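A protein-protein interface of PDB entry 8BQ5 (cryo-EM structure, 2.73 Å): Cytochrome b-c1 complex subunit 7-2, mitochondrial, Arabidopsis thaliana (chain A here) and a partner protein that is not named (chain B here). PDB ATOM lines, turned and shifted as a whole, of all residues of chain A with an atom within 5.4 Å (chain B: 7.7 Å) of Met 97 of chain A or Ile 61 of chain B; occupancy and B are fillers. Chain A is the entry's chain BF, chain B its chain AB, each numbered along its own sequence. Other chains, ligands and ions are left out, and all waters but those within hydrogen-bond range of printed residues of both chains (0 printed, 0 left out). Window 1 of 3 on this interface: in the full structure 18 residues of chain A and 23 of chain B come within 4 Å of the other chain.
The side-chain carboxylate (OE1) of Glu 59 of chain B is in salt-bridge range of the side-chain amino group (NZ) of Lys 62 of chain B (3.4 Å).
Hydrophobic or aromatic side chains of chain B that line the printed part of chain A: Ala 57, Ala 58, Ile 61 and Ile 65.
Of the 16 printed residues of chain A, 3 touch a printed residue of chain B.
Hydrophobic or aromatic side chains of chain A within 4 Å of the printed part of chain B: Ile 58 and Met 97.
Along chain A the printed residues that touch a printed residue of chain B span positions 58 to 97.
Among the printed residues, no Asp or Glu carboxylate lies within 4 Å of a Lys or Arg side-chain nitrogen of the other chain.
Among the printed residues, pairs that only touch across the chains: Ile 58 of chain A with Tyr 54 of chain B, Ile 58 of chain A with Ala 58 of chain B, Ile 58 of chain A with Ala 57 of chain B, Met 97 of chain A with Ile 65 of chain B, Asp 96 of chain A with Lys 62 of chain B, Met 97 of chain A with Ile 61 of chain B, Asp 96 of chain A with Lys 66 of chain B and Asp 96 of chain A with Ile 65 of chain B.
Met 97 of chain A touches just these residues of chain B: Ile 61 (3.8 Å) and Ile 65 (3.6 Å).
Of the printed residues of chain A, Ile 61 of chain B touches Met 97 (3.8 Å).
Of the printed residues of chain A, Ile 65 of chain B touches Asp 96 (3.8 Å) and Met 97 (3.6 Å).
Printed residues of chain B within 4 Å of Ile 58 of chain A: Tyr 54, Ala 57 and Ala 58.
Printed residues of chain A within 4 Å of Ala 58 of chain B: Ile 58 (3.5 Å).
Printed residues of chain A within 4 Å of Tyr 54 of chain B: Ile 58 (3.3 Å).
Of the printed residues of chain B, Asp 96 of chain A touches Lys 62, Ile 65 and Lys 66.
The nearest residue of chain B that does not touch Met 97 of chain A is Lys 62 of chain B (6.1 Å).
The nearest residue of chain A that does not touch Ile 61 of chain B is Pro 55 of chain A (4.3 Å).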
ATOM      1  N   ALA A  50       2.172 -21.478  18.258  1.00  0.00           N
ATOM      2  CA  ALA A  50       3.024 -20.445  18.836  1.00  0.00           C
ATOM      3  C   ALA A  50       3.222 -20.666  20.329  1.00  0.00           C
ATOM      4  O   ALA A  50       4.332 -20.501  20.846  1.00  0.00           O
ATOM      5  CB  ALA A  50       2.428 -19.064  18.571  1.00  0.00           C
ATOM      6  N   LEU A  51       2.154 -21.039  21.037  1.00  0.00           N
ATOM      7  CA  LEU A  51       2.265 -21.295  22.470  1.00  0.00           C
ATOM      8  C   LEU A  51       3.159 -22.496  22.753  1.00  0.00           C
ATOM      9  O   LEU A  51       3.937 -22.482  23.713  1.00  0.00           O
ATOM     10  CB  LEU A  51       0.877 -21.507  23.072  1.00  0.00           C
ATOM     11  CG  LEU A  51       0.639 -20.962  24.481  1.00  0.00           C
ATOM     12  CD1 LEU A  51       0.362 -19.468  24.449  1.00  0.00           C
ATOM     13  CD2 LEU A  51      -0.504 -21.707  25.140  1.00  0.00           C
ATOM     14  N   ARG A  53       5.688 -23.451  21.153  1.00  0.00           N
ATOM     15  CA  ARG A  53       7.081 -23.109  20.903  1.00  0.00           C
ATOM     16  C   ARG A  53       7.676 -22.207  21.977  1.00  0.00           C
ATOM     17  O   ARG A  53       8.901 -22.046  22.015  1.00  0.00           O
ATOM     18  CB  ARG A  53       7.213 -22.433  19.538  1.00  0.00           C
ATOM     19  CG  ARG A  53       7.180 -23.398  18.371  1.00  0.00           C
ATOM     20  CD  ARG A  53       7.306 -22.670  17.047  1.00  0.00           C
ATOM     21  NE  ARG A  53       6.863 -23.494  15.931  1.00  0.00           N
ATOM     22  CZ  ARG A  53       7.068 -23.197  14.654  1.00  0.00           C
ATOM     23  NH1 ARG A  53       7.720 -22.103  14.297  1.00  0.00           N
ATOM     24  NH2 ARG A  53       6.609 -24.019  13.715  1.00  0.00           N
ATOM     25  N   LEU A  54       6.853 -21.625  22.841  1.00  0.00           N
ATOM     26  CA  LEU A  54       7.342 -20.725  23.870  1.00  0.00           C
ATOM     27  C   LEU A  54       7.990 -21.508  25.009  1.00  0.00           C
ATOM     28  O   LEU A  54       7.647 -22.667  25.256  1.00  0.00           O
ATOM     29  CB  LEU A  54       6.199 -19.871  24.409  1.00  0.00           C
ATOM     30  CG  LEU A  54       5.655 -18.771  23.495  1.00  0.00           C
ATOM     31  CD1 LEU A  54       4.379 -18.187  24.078  1.00  0.00           C
ATOM     32  CD2 LEU A  54       6.693 -17.683  23.274  1.00  0.00           C
ATOM     33  N   PRO A  55       8.934 -20.892  25.719  1.00  0.00           N
ATOM     34  CA  PRO A  55       9.556 -21.574  26.859  1.00  0.00           C
ATOM     35  C   PRO A  55       8.549 -21.850  27.963  1.00  0.00           C
ATOM     36  O   PRO A  55       7.512 -21.192  28.072  1.00  0.00           O
ATOM     37  CB  PRO A  55      10.635 -20.587  27.317  1.00  0.00           C
ATOM     38  CG  PRO A  55      10.936 -19.776  26.106  1.00  0.00           C
ATOM     39  CD  PRO A  55       9.630 -19.640  25.381  1.00  0.00           C
ATOM     40  N   ILE A  58       7.416 -19.030  30.541  1.00  0.00           N
ATOM     41  CA  ILE A  58       6.428 -18.065  30.062  1.00  0.00           C
ATOM     42  C   ILE A  58       5.031 -18.671  30.074  1.00  0.00           C
ATOM     43  O   ILE A  58       4.063 -18.027  30.500  1.00  0.00           O
ATOM     44  CB  ILE A  58       6.812 -17.549  28.663  1.00  0.00           C
ATOM     45  CG1 ILE A  58       8.084 -16.712  28.745  1.00  0.00           C
ATOM     46  CG2 ILE A  58       5.682 -16.736  28.056  1.00  0.00           C
ATOM     47  CD1 ILE A  58       9.282 -17.394  28.189  1.00  0.00           C
ATOM     48  N   TYR A  93       4.511 -11.320  24.995  1.00  0.00           N
ATOM     49  CA  TYR A  93       5.287 -12.553  24.947  1.00  0.00           C
ATOM     50  C   TYR A  93       4.906 -13.466  23.793  1.00  0.00           C
ATOM     51  O   TYR A  93       5.568 -14.492  23.610  1.00  0.00           O
ATOM     52  CB  TYR A  93       5.150 -13.333  26.265  1.00  0.00           C
ATOM     53  CG  TYR A  93       3.742 -13.798  26.574  1.00  0.00           C
ATOM     54  CD1 TYR A  93       3.258 -14.999  26.070  1.00  0.00           C
ATOM     55  CD2 TYR A  93       2.901 -13.038  27.372  1.00  0.00           C
ATOM     56  CE1 TYR A  93       1.977 -15.425  26.347  1.00  0.00           C
ATOM     57  CE2 TYR A  93       1.617 -13.458  27.657  1.00  0.00           C
ATOM     58  CZ  TYR A  93       1.162 -14.652  27.141  1.00  0.00           C
ATOM     59  OH  TYR A  93      -0.115 -15.077  27.420  1.00  0.00           O
ATOM     60  N   LEU A  94       3.843 -13.144  23.048  1.00  0.00           N
ATOM     61  CA  LEU A  94       3.334 -14.102  22.026  1.00  0.00           C
ATOM     62  C   LEU A  94       3.340 -13.522  20.612  1.00  0.00           C
ATOM     63  O   LEU A  94       3.630 -14.290  19.690  1.00  0.00           O
ATOM     64  CB  LEU A  94       1.908 -14.482  22.435  1.00  0.00           C
ATOM     65  CG  LEU A  94       1.158 -15.429  21.500  1.00  0.00           C
ATOM     66  CD1 LEU A  94       1.669 -16.852  21.640  1.00  0.00           C
ATOM     67  CD2 LEU A  94      -0.336 -15.372  21.767  1.00  0.00           C
ATOM     68  N   GLN A  95       3.067 -12.231  20.444  1.00  0.00           N
ATOM     69  CA  GLN A  95       2.910 -11.650  19.079  1.00  0.00           C
ATOM     70  C   GLN A  95       4.090 -11.972  18.146  1.00  0.00           C
ATOM     71  O   GLN A  95       3.814 -12.294  16.984  1.00  0.00           O
ATOM     72  CB  GLN A  95       2.622 -10.153  19.181  1.00  0.00           C
ATOM     73  CG  GLN A  95       1.331  -9.860  19.926  1.00  0.00           C
ATOM     74  CD  GLN A  95       0.150 -10.660  19.426  1.00  0.00           C
ATOM     75  OE1 GLN A  95      -0.248 -10.564  18.267  1.00  0.00           O
ATOM     76  NE2 GLN A  95      -0.434 -11.448  20.313  1.00  0.00           N
ATOM     77  N   ASP A  96       5.338 -11.869  18.608  1.00  0.00           N
ATOM     78  CA  ASP A  96       6.473 -12.149  17.731  1.00  0.00           C
ATOM     79  C   ASP A  96       6.493 -13.609  17.295  1.00  0.00           C
ATOM     80  O   ASP A  96       6.725 -13.906  16.117  1.00  0.00           O
ATOM     81  CB  ASP A  96       7.780 -11.778  18.427  1.00  0.00           C
ATOM     82  CG  ASP A  96       7.951 -10.282  18.587  1.00  0.00           C
ATOM     83  OD1 ASP A  96       9.037  -9.851  19.025  1.00  0.00           O
ATOM     84  OD2 ASP A  96       6.998  -9.537  18.275  1.00  0.00           O
ATOM     85  N   MET A  97       6.260 -14.532  18.228  1.00  0.00           N
ATOM     86  CA  MET A  97       6.218 -15.947  17.875  1.00  0.00           C
ATOM     87  C   MET A  97       5.024 -16.257  16.982  1.00  0.00           C
ATOM     88  O   MET A  97       5.134 -17.055  16.044  1.00  0.00           O
ATOM     89  CB  MET A  97       6.185 -16.804  19.139  1.00  0.00           C
ATOM     90  CG  MET A  97       6.215 -18.299  18.875  1.00  0.00           C
ATOM     91  SD  MET A  97       7.792 -18.864  18.212  1.00  0.00           S
ATOM     92  CE  MET A  97       8.766 -18.973  19.709  1.00  0.00           C
ATOM     93  N   LEU A  98       3.873 -15.652  17.278  1.00  0.00           N
ATOM     94  CA  LEU A  98       2.668 -15.846  16.431  1.00  0.00           C
ATOM     95  C   LEU A  98       2.976 -15.373  15.006  1.00  0.00           C
ATOM     96  O   LEU A  98       2.638 -16.106  14.072  1.00  0.00           O
ATOM     97  CB  LEU A  98       1.492 -15.079  17.040  1.00  0.00           C
ATOM     98  CG  LEU A  98       0.144 -15.265  16.349  1.00  0.00           C
ATOM     99  CD1 LEU A  98      -0.225 -16.736  16.256  1.00  0.00           C
ATOM    100  CD2 LEU A  98      -0.943 -14.490  17.074  1.00  0.00           C
ATOM    101  N   ALA A  99       3.614 -14.211  14.854  1.00  0.00           N
ATOM    102  CA  ALA A  99       3.917 -13.696  13.523  1.00  0.00           C
ATOM    103  C   ALA A  99       4.867 -14.624  12.773  1.00  0.00           C
ATOM    104  O   ALA A  99       4.717 -14.830  11.564  1.00  0.00           O
ATOM    105  CB  ALA A  99       4.508 -12.290  13.624  1.00  0.00           C
ATOM    106  N   LEU A 100       5.859 -15.179  13.473  1.00  0.00           N
ATOM    107  CA  LEU A 100       6.780 -16.116  12.839  1.00  0.00           C
ATOM    108  C   LEU A 100       6.061 -17.383  12.391  1.00  0.00           C
ATOM    109  O   LEU A 100       6.326 -17.903  11.301  1.00  0.00           O
ATOM    110  CB  LEU A 100       7.920 -16.457  13.797  1.00  0.00           C
ATOM    111  CG  LEU A 100       8.862 -17.578  13.353  1.00  0.00           C
ATOM    112  CD1 LEU A 100       9.786 -17.097  12.248  1.00  0.00           C
ATOM    113  CD2 LEU A 100       9.658 -18.104  14.532  1.00  0.00           C
ATOM    114  N   VAL A 101       5.149 -17.894  13.221  1.00  0.00           N
ATOM    115  CA  VAL A 101       4.394 -19.090  12.862  1.00  0.00           C
ATOM    116  C   VAL A 101       3.536 -18.826  11.630  1.00  0.00           C
ATOM    117  O   VAL A 101       3.425 -19.675  10.737  1.00  0.00           O
ATOM    118  CB  VAL A 101       3.549 -19.563  14.061  1.00  0.00           C
ATOM    119  CG1 VAL A 101       2.410 -20.455  13.602  1.00  0.00           C
ATOM    120  CG2 VAL A 101       4.424 -20.286  15.070  1.00  0.00           C
ATOM    121  N   LYS A 102       2.921 -17.643  11.560  1.00  0.00           N
ATOM    122  CA  LYS A 102       2.142 -17.276  10.383  1.00  0.00           C
ATOM    123  C   LYS A 102       3.025 -17.151   9.147  1.00  0.00           C
ATOM    124  O   LYS A 102       2.613 -17.524   8.042  1.00  0.00           O
ATOM    125  CB  LYS A 102       1.392 -15.969  10.639  1.00  0.00           C
ATOM    126  CG  LYS A 102       0.341 -16.063  11.731  1.00  0.00           C
ATOM    127  CD  LYS A 102      -0.760 -15.033  11.539  1.00  0.00           C
ATOM    128  CE  LYS A 102      -0.526 -13.807  12.409  1.00  0.00           C
ATOM    129  NZ  LYS A 102       0.727 -13.088  12.051  1.00  0.00           N
ATOM    130  N   TYR B  54      10.164 -15.207  34.199  1.00  0.00           N
ATOM    131  CA  TYR B  54       9.390 -15.449  32.987  1.00  0.00           C
ATOM    132  C   TYR B  54       9.486 -14.271  32.026  1.00  0.00           C
ATOM    133  O   TYR B  54       9.416 -14.452  30.806  1.00  0.00           O
ATOM    134  CB  TYR B  54       7.931 -15.748  33.334  1.00  0.00           C
ATOM    135  CG  TYR B  54       7.323 -14.820  34.359  1.00  0.00           C
ATOM    136  CD1 TYR B  54       6.749 -13.616  33.978  1.00  0.00           C
ATOM    137  CD2 TYR B  54       7.309 -15.157  35.705  1.00  0.00           C
ATOM    138  CE1 TYR B  54       6.188 -12.768  34.910  1.00  0.00           C
ATOM    139  CE2 TYR B  54       6.751 -14.316  36.643  1.00  0.00           C
ATOM    140  CZ  TYR B  54       6.191 -13.124  36.241  1.00  0.00           C
ATOM    141  OH  TYR B  54       5.632 -12.284  37.174  1.00  0.00           O
ATOM    142  N   ASP B  55       9.636 -13.056  32.557  1.00  0.00           N
ATOM    143  CA  ASP B  55       9.801 -11.894  31.691  1.00  0.00           C
ATOM    144  C   ASP B  55      11.162 -11.908  31.006  1.00  0.00           C
ATOM    145  O   ASP B  55      11.272 -11.570  29.822  1.00  0.00           O
ATOM    146  CB  ASP B  55       9.616 -10.609  32.496  1.00  0.00           C
ATOM    147  CG  ASP B  55       8.161 -10.240  32.666  1.00  0.00           C
ATOM    148  OD1 ASP B  55       7.325 -10.738  31.884  1.00  0.00           O
ATOM    149  OD2 ASP B  55       7.850  -9.451  33.582  1.00  0.00           O
ATOM    150  N   HIS B  56      12.209 -12.293  31.738  1.00  0.00           N
ATOM    151  CA  HIS B  56      13.538 -12.374  31.143  1.00  0.00           C
ATOM    152  C   HIS B  56      13.584 -13.413  30.031  1.00  0.00           C
ATOM    153  O   HIS B  56      14.179 -13.175  28.972  1.00  0.00           O
ATOM    154  CB  HIS B  56      14.573 -12.698  32.220  1.00  0.00           C
ATOM    155  CG  HIS B  56      15.930 -13.017  31.678  1.00  0.00           C
ATOM    156  ND1 HIS B  56      16.706 -12.087  31.020  1.00  0.00           N
ATOM    157  CD2 HIS B  56      16.647 -14.165  31.690  1.00  0.00           C
ATOM    158  CE1 HIS B  56      17.844 -12.647  30.654  1.00  0.00           C
ATOM    159  NE2 HIS B  56      17.834 -13.908  31.050  1.00  0.00           N
ATOM    160  N   ALA B  57      12.961 -14.571  30.251  1.00  0.00           N
ATOM    161  CA  ALA B  57      12.967 -15.618  29.235  1.00  0.00           C
ATOM    162  C   ALA B  57      12.173 -15.199  28.004  1.00  0.00           C
ATOM    163  O   ALA B  57      12.498 -15.601  26.881  1.00  0.00           O
ATOM    164  CB  ALA B  57      12.415 -16.916  29.820  1.00  0.00           C
ATOM    165  N   ALA B  58      11.125 -14.396  28.195  1.00  0.00           N
ATOM    166  CA  ALA B  58      10.355 -13.908  27.056  1.00  0.00           C
ATOM    167  C   ALA B  58      11.170 -12.935  26.215  1.00  0.00           C
ATOM    168  O   ALA B  58      11.015 -12.881  24.989  1.00  0.00           O
ATOM    169  CB  ALA B  58       9.061 -13.253  27.537  1.00  0.00           C
ATOM    170  N   GLU B  59      12.035 -12.145  26.856  1.00  0.00           N
ATOM    171  CA  GLU B  59      12.886 -11.224  26.109  1.00  0.00           C
ATOM    172  C   GLU B  59      13.896 -11.975  25.252  1.00  0.00           C
ATOM    173  O   GLU B  59      14.189 -11.565  24.124  1.00  0.00           O
ATOM    174  CB  GLU B  59      13.601 -10.270  27.066  1.00  0.00           C
ATOM    175  CG  GLU B  59      12.699  -9.235  27.722  1.00  0.00           C
ATOM    176  CD  GLU B  59      12.210  -8.176  26.750  1.00  0.00           C
ATOM    177  OE1 GLU B  59      11.294  -8.468  25.956  1.00  0.00           O
ATOM    178  OE2 GLU B  59      12.745  -7.048  26.781  1.00  0.00           O
ATOM    179  N   ILE B  60      14.446 -13.072  25.775  1.00  0.00           N
ATOM    180  CA  ILE B  60      15.439 -13.839  25.026  1.00  0.00           C
ATOM    181  C   ILE B  60      14.824 -14.411  23.755  1.00  0.00           C
ATOM    182  O   ILE B  60      15.396 -14.300  22.664  1.00  0.00           O
ATOM    183  CB  ILE B  60      16.039 -14.950  25.908  1.00  0.00           C
ATOM    184  CG1 ILE B  60      17.014 -14.357  26.923  1.00  0.00           C
ATOM    185  CG2 ILE B  60      16.732 -15.997  25.055  1.00  0.00           C
ATOM    186  CD1 ILE B  60      17.219 -15.229  28.131  1.00  0.00           C
ATOM    187  N   ILE B  61      13.646 -15.028  23.874  1.00  0.00           N
ATOM    188  CA  ILE B  61      13.025 -15.654  22.712  1.00  0.00           C
ATOM    189  C   ILE B  61      12.555 -14.596  21.719  1.00  0.00           C
ATOM    190  O   ILE B  61      12.545 -14.828  20.504  1.00  0.00           O
ATOM    191  CB  ILE B  61      11.882 -16.591  23.148  1.00  0.00           C
ATOM    192  CG1 ILE B  61      11.385 -17.418  21.960  1.00  0.00           C
ATOM    193  CG2 ILE B  61      10.734 -15.814  23.760  1.00  0.00           C
ATOM    194  CD1 ILE B  61      12.231 -18.635  21.672  1.00  0.00           C
ATOM    195  N   LYS B  62      12.162 -13.420  22.214  1.00  0.00           N
ATOM    196  CA  LYS B  62      11.776 -12.341  21.313  1.00  0.00           C
ATOM    197  C   LYS B  62      12.981 -11.800  20.557  1.00  0.00           C
ATOM    198  O   LYS B  62      12.868 -11.406  19.390  1.00  0.00           O
ATOM    199  CB  LYS B  62      11.082 -11.226  22.094  1.00  0.00           C
ATOM    200  CG  LYS B  62       9.602 -11.472  22.334  1.00  0.00           C
ATOM    201  CD  LYS B  62       8.889 -10.192  22.729  1.00  0.00           C
ATOM    202  CE  LYS B  62       9.082  -9.894  24.202  1.00  0.00           C
ATOM    203  NZ  LYS B  62       8.164  -8.824  24.677  1.00  0.00           N
ATOM    204  N   ASN B  63      14.146 -11.766  21.209  1.00  0.00           N
ATOM    205  CA  ASN B  63      15.360 -11.325  20.531  1.00  0.00           C
ATOM    206  C   ASN B  63      15.807 -12.336  19.484  1.00  0.00           C
ATOM    207  O   ASN B  63      16.278 -11.955  18.407  1.00  0.00           O
ATOM    208  CB  ASN B  63      16.470 -11.084  21.553  1.00  0.00           C
ATOM    209  CG  ASN B  63      16.399  -9.704  22.168  1.00  0.00           C
ATOM    210  OD1 ASN B  63      15.568  -8.883  21.783  1.00  0.00           O
ATOM    211  ND2 ASN B  63      17.271  -9.442  23.134  1.00  0.00           N
ATOM    212  N   LYS B  64      15.676 -13.628  19.787  1.00  0.00           N
ATOM    213  CA  LYS B  64      16.022 -14.653  18.808  1.00  0.00           C
ATOM    214  C   LYS B  64      15.128 -14.557  17.579  1.00  0.00           C
ATOM    215  O   LYS B  64      15.592 -14.736  16.447  1.00  0.00           O
ATOM    216  CB  LYS B  64      15.915 -16.037  19.446  1.00  0.00           C
ATOM    217  CG  LYS B  64      16.911 -17.052  18.919  1.00  0.00           C
ATOM    218  CD  LYS B  64      16.353 -18.462  19.020  1.00  0.00           C
ATOM    219  CE  LYS B  64      17.454 -19.506  18.943  1.00  0.00           C
ATOM    220  NZ  LYS B  64      18.575 -19.072  18.066  1.00  0.00           N
ATOM    221  N   ILE B  65      13.843 -14.268  17.785  1.00  0.00           N
ATOM    222  CA  ILE B  65      12.904 -14.176  16.672  1.00  0.00           C
ATOM    223  C   ILE B  65      13.232 -12.979  15.786  1.00  0.00           C
ATOM    224  O   ILE B  65      13.167 -13.067  14.553  1.00  0.00           O
ATOM    225  CB  ILE B  65      11.463 -14.123  17.210  1.00  0.00           C
ATOM    226  CG1 ILE B  65      10.931 -15.540  17.412  1.00  0.00           C
ATOM    227  CG2 ILE B  65      10.556 -13.345  16.271  1.00  0.00           C
ATOM    228  CD1 ILE B  65       9.788 -15.621  18.385  1.00  0.00           C
ATOM    229  N   LYS B  66      13.589 -11.843  16.391  1.00  0.00           N
ATOM    230  CA  LYS B  66      13.962 -10.673  15.601  1.00  0.00           C
ATOM    231  C   LYS B  66      15.229 -10.943  14.797  1.00  0.00           C
ATOM    232  O   LYS B  66      15.395 -10.427  13.687  1.00  0.00           O
ATOM    233  CB  LYS B  66      14.125  -9.453  16.518  1.00  0.00           C
ATOM    234  CG  LYS B  66      12.851  -8.931  17.193  1.00  0.00           C
ATOM    235  CD  LYS B  66      13.102  -7.731  18.108  1.00  0.00           C
ATOM    236  CE  LYS B  66      11.817  -7.225  18.739  1.00  0.00           C
ATOM    237  NZ  LYS B  66      12.066  -6.072  19.649  1.00  0.00           N
ATOM    238  N   LYS B  67      16.131 -11.760  15.344  1.00  0.00           N
ATOM    239  CA  LYS B  67      17.331 -12.150  14.612  1.00  0.00           C
ATOM    240  C   LYS B  67      16.974 -12.908  13.339  1.00  0.00           C
ATOM    241  O   LYS B  67      17.601 -12.712  12.292  1.00  0.00           O
ATOM    242  CB  LYS B  67      18.232 -12.995  15.515  1.00  0.00           C
ATOM    243  CG  LYS B  67      19.678 -13.105  15.069  1.00  0.00           C
ATOM    244  CD  LYS B  67      20.539 -13.649  16.200  1.00  0.00           C
ATOM    245  CE  LYS B  67      21.524 -14.694  15.705  1.00  0.00           C
ATOM    246  NZ  LYS B  67      22.892 -14.470  16.249  1.00  0.00           N
ATOM    247  N   LEU B  68      15.964 -13.778  13.409  1.00  0.00           N
ATOM    248  CA  LEU B  68      15.505 -14.496  12.224  1.00  0.00           C
ATOM    249  C   LEU B  68      14.694 -13.614  11.286  1.00  0.00           C
ATOM    250  O   LEU B  68      14.465 -14.002  10.137  1.00  0.00           O
ATOM    251  CB  LEU B  68      14.667 -15.706  12.632  1.00  0.00           C
ATOM    252  CG  LEU B  68      15.300 -16.698  13.605  1.00  0.00           C
ATOM    253  CD1 LEU B  68      14.237 -17.623  14.165  1.00  0.00           C
ATOM    254  CD2 LEU B  68      16.396 -17.490  12.917  1.00  0.00           C
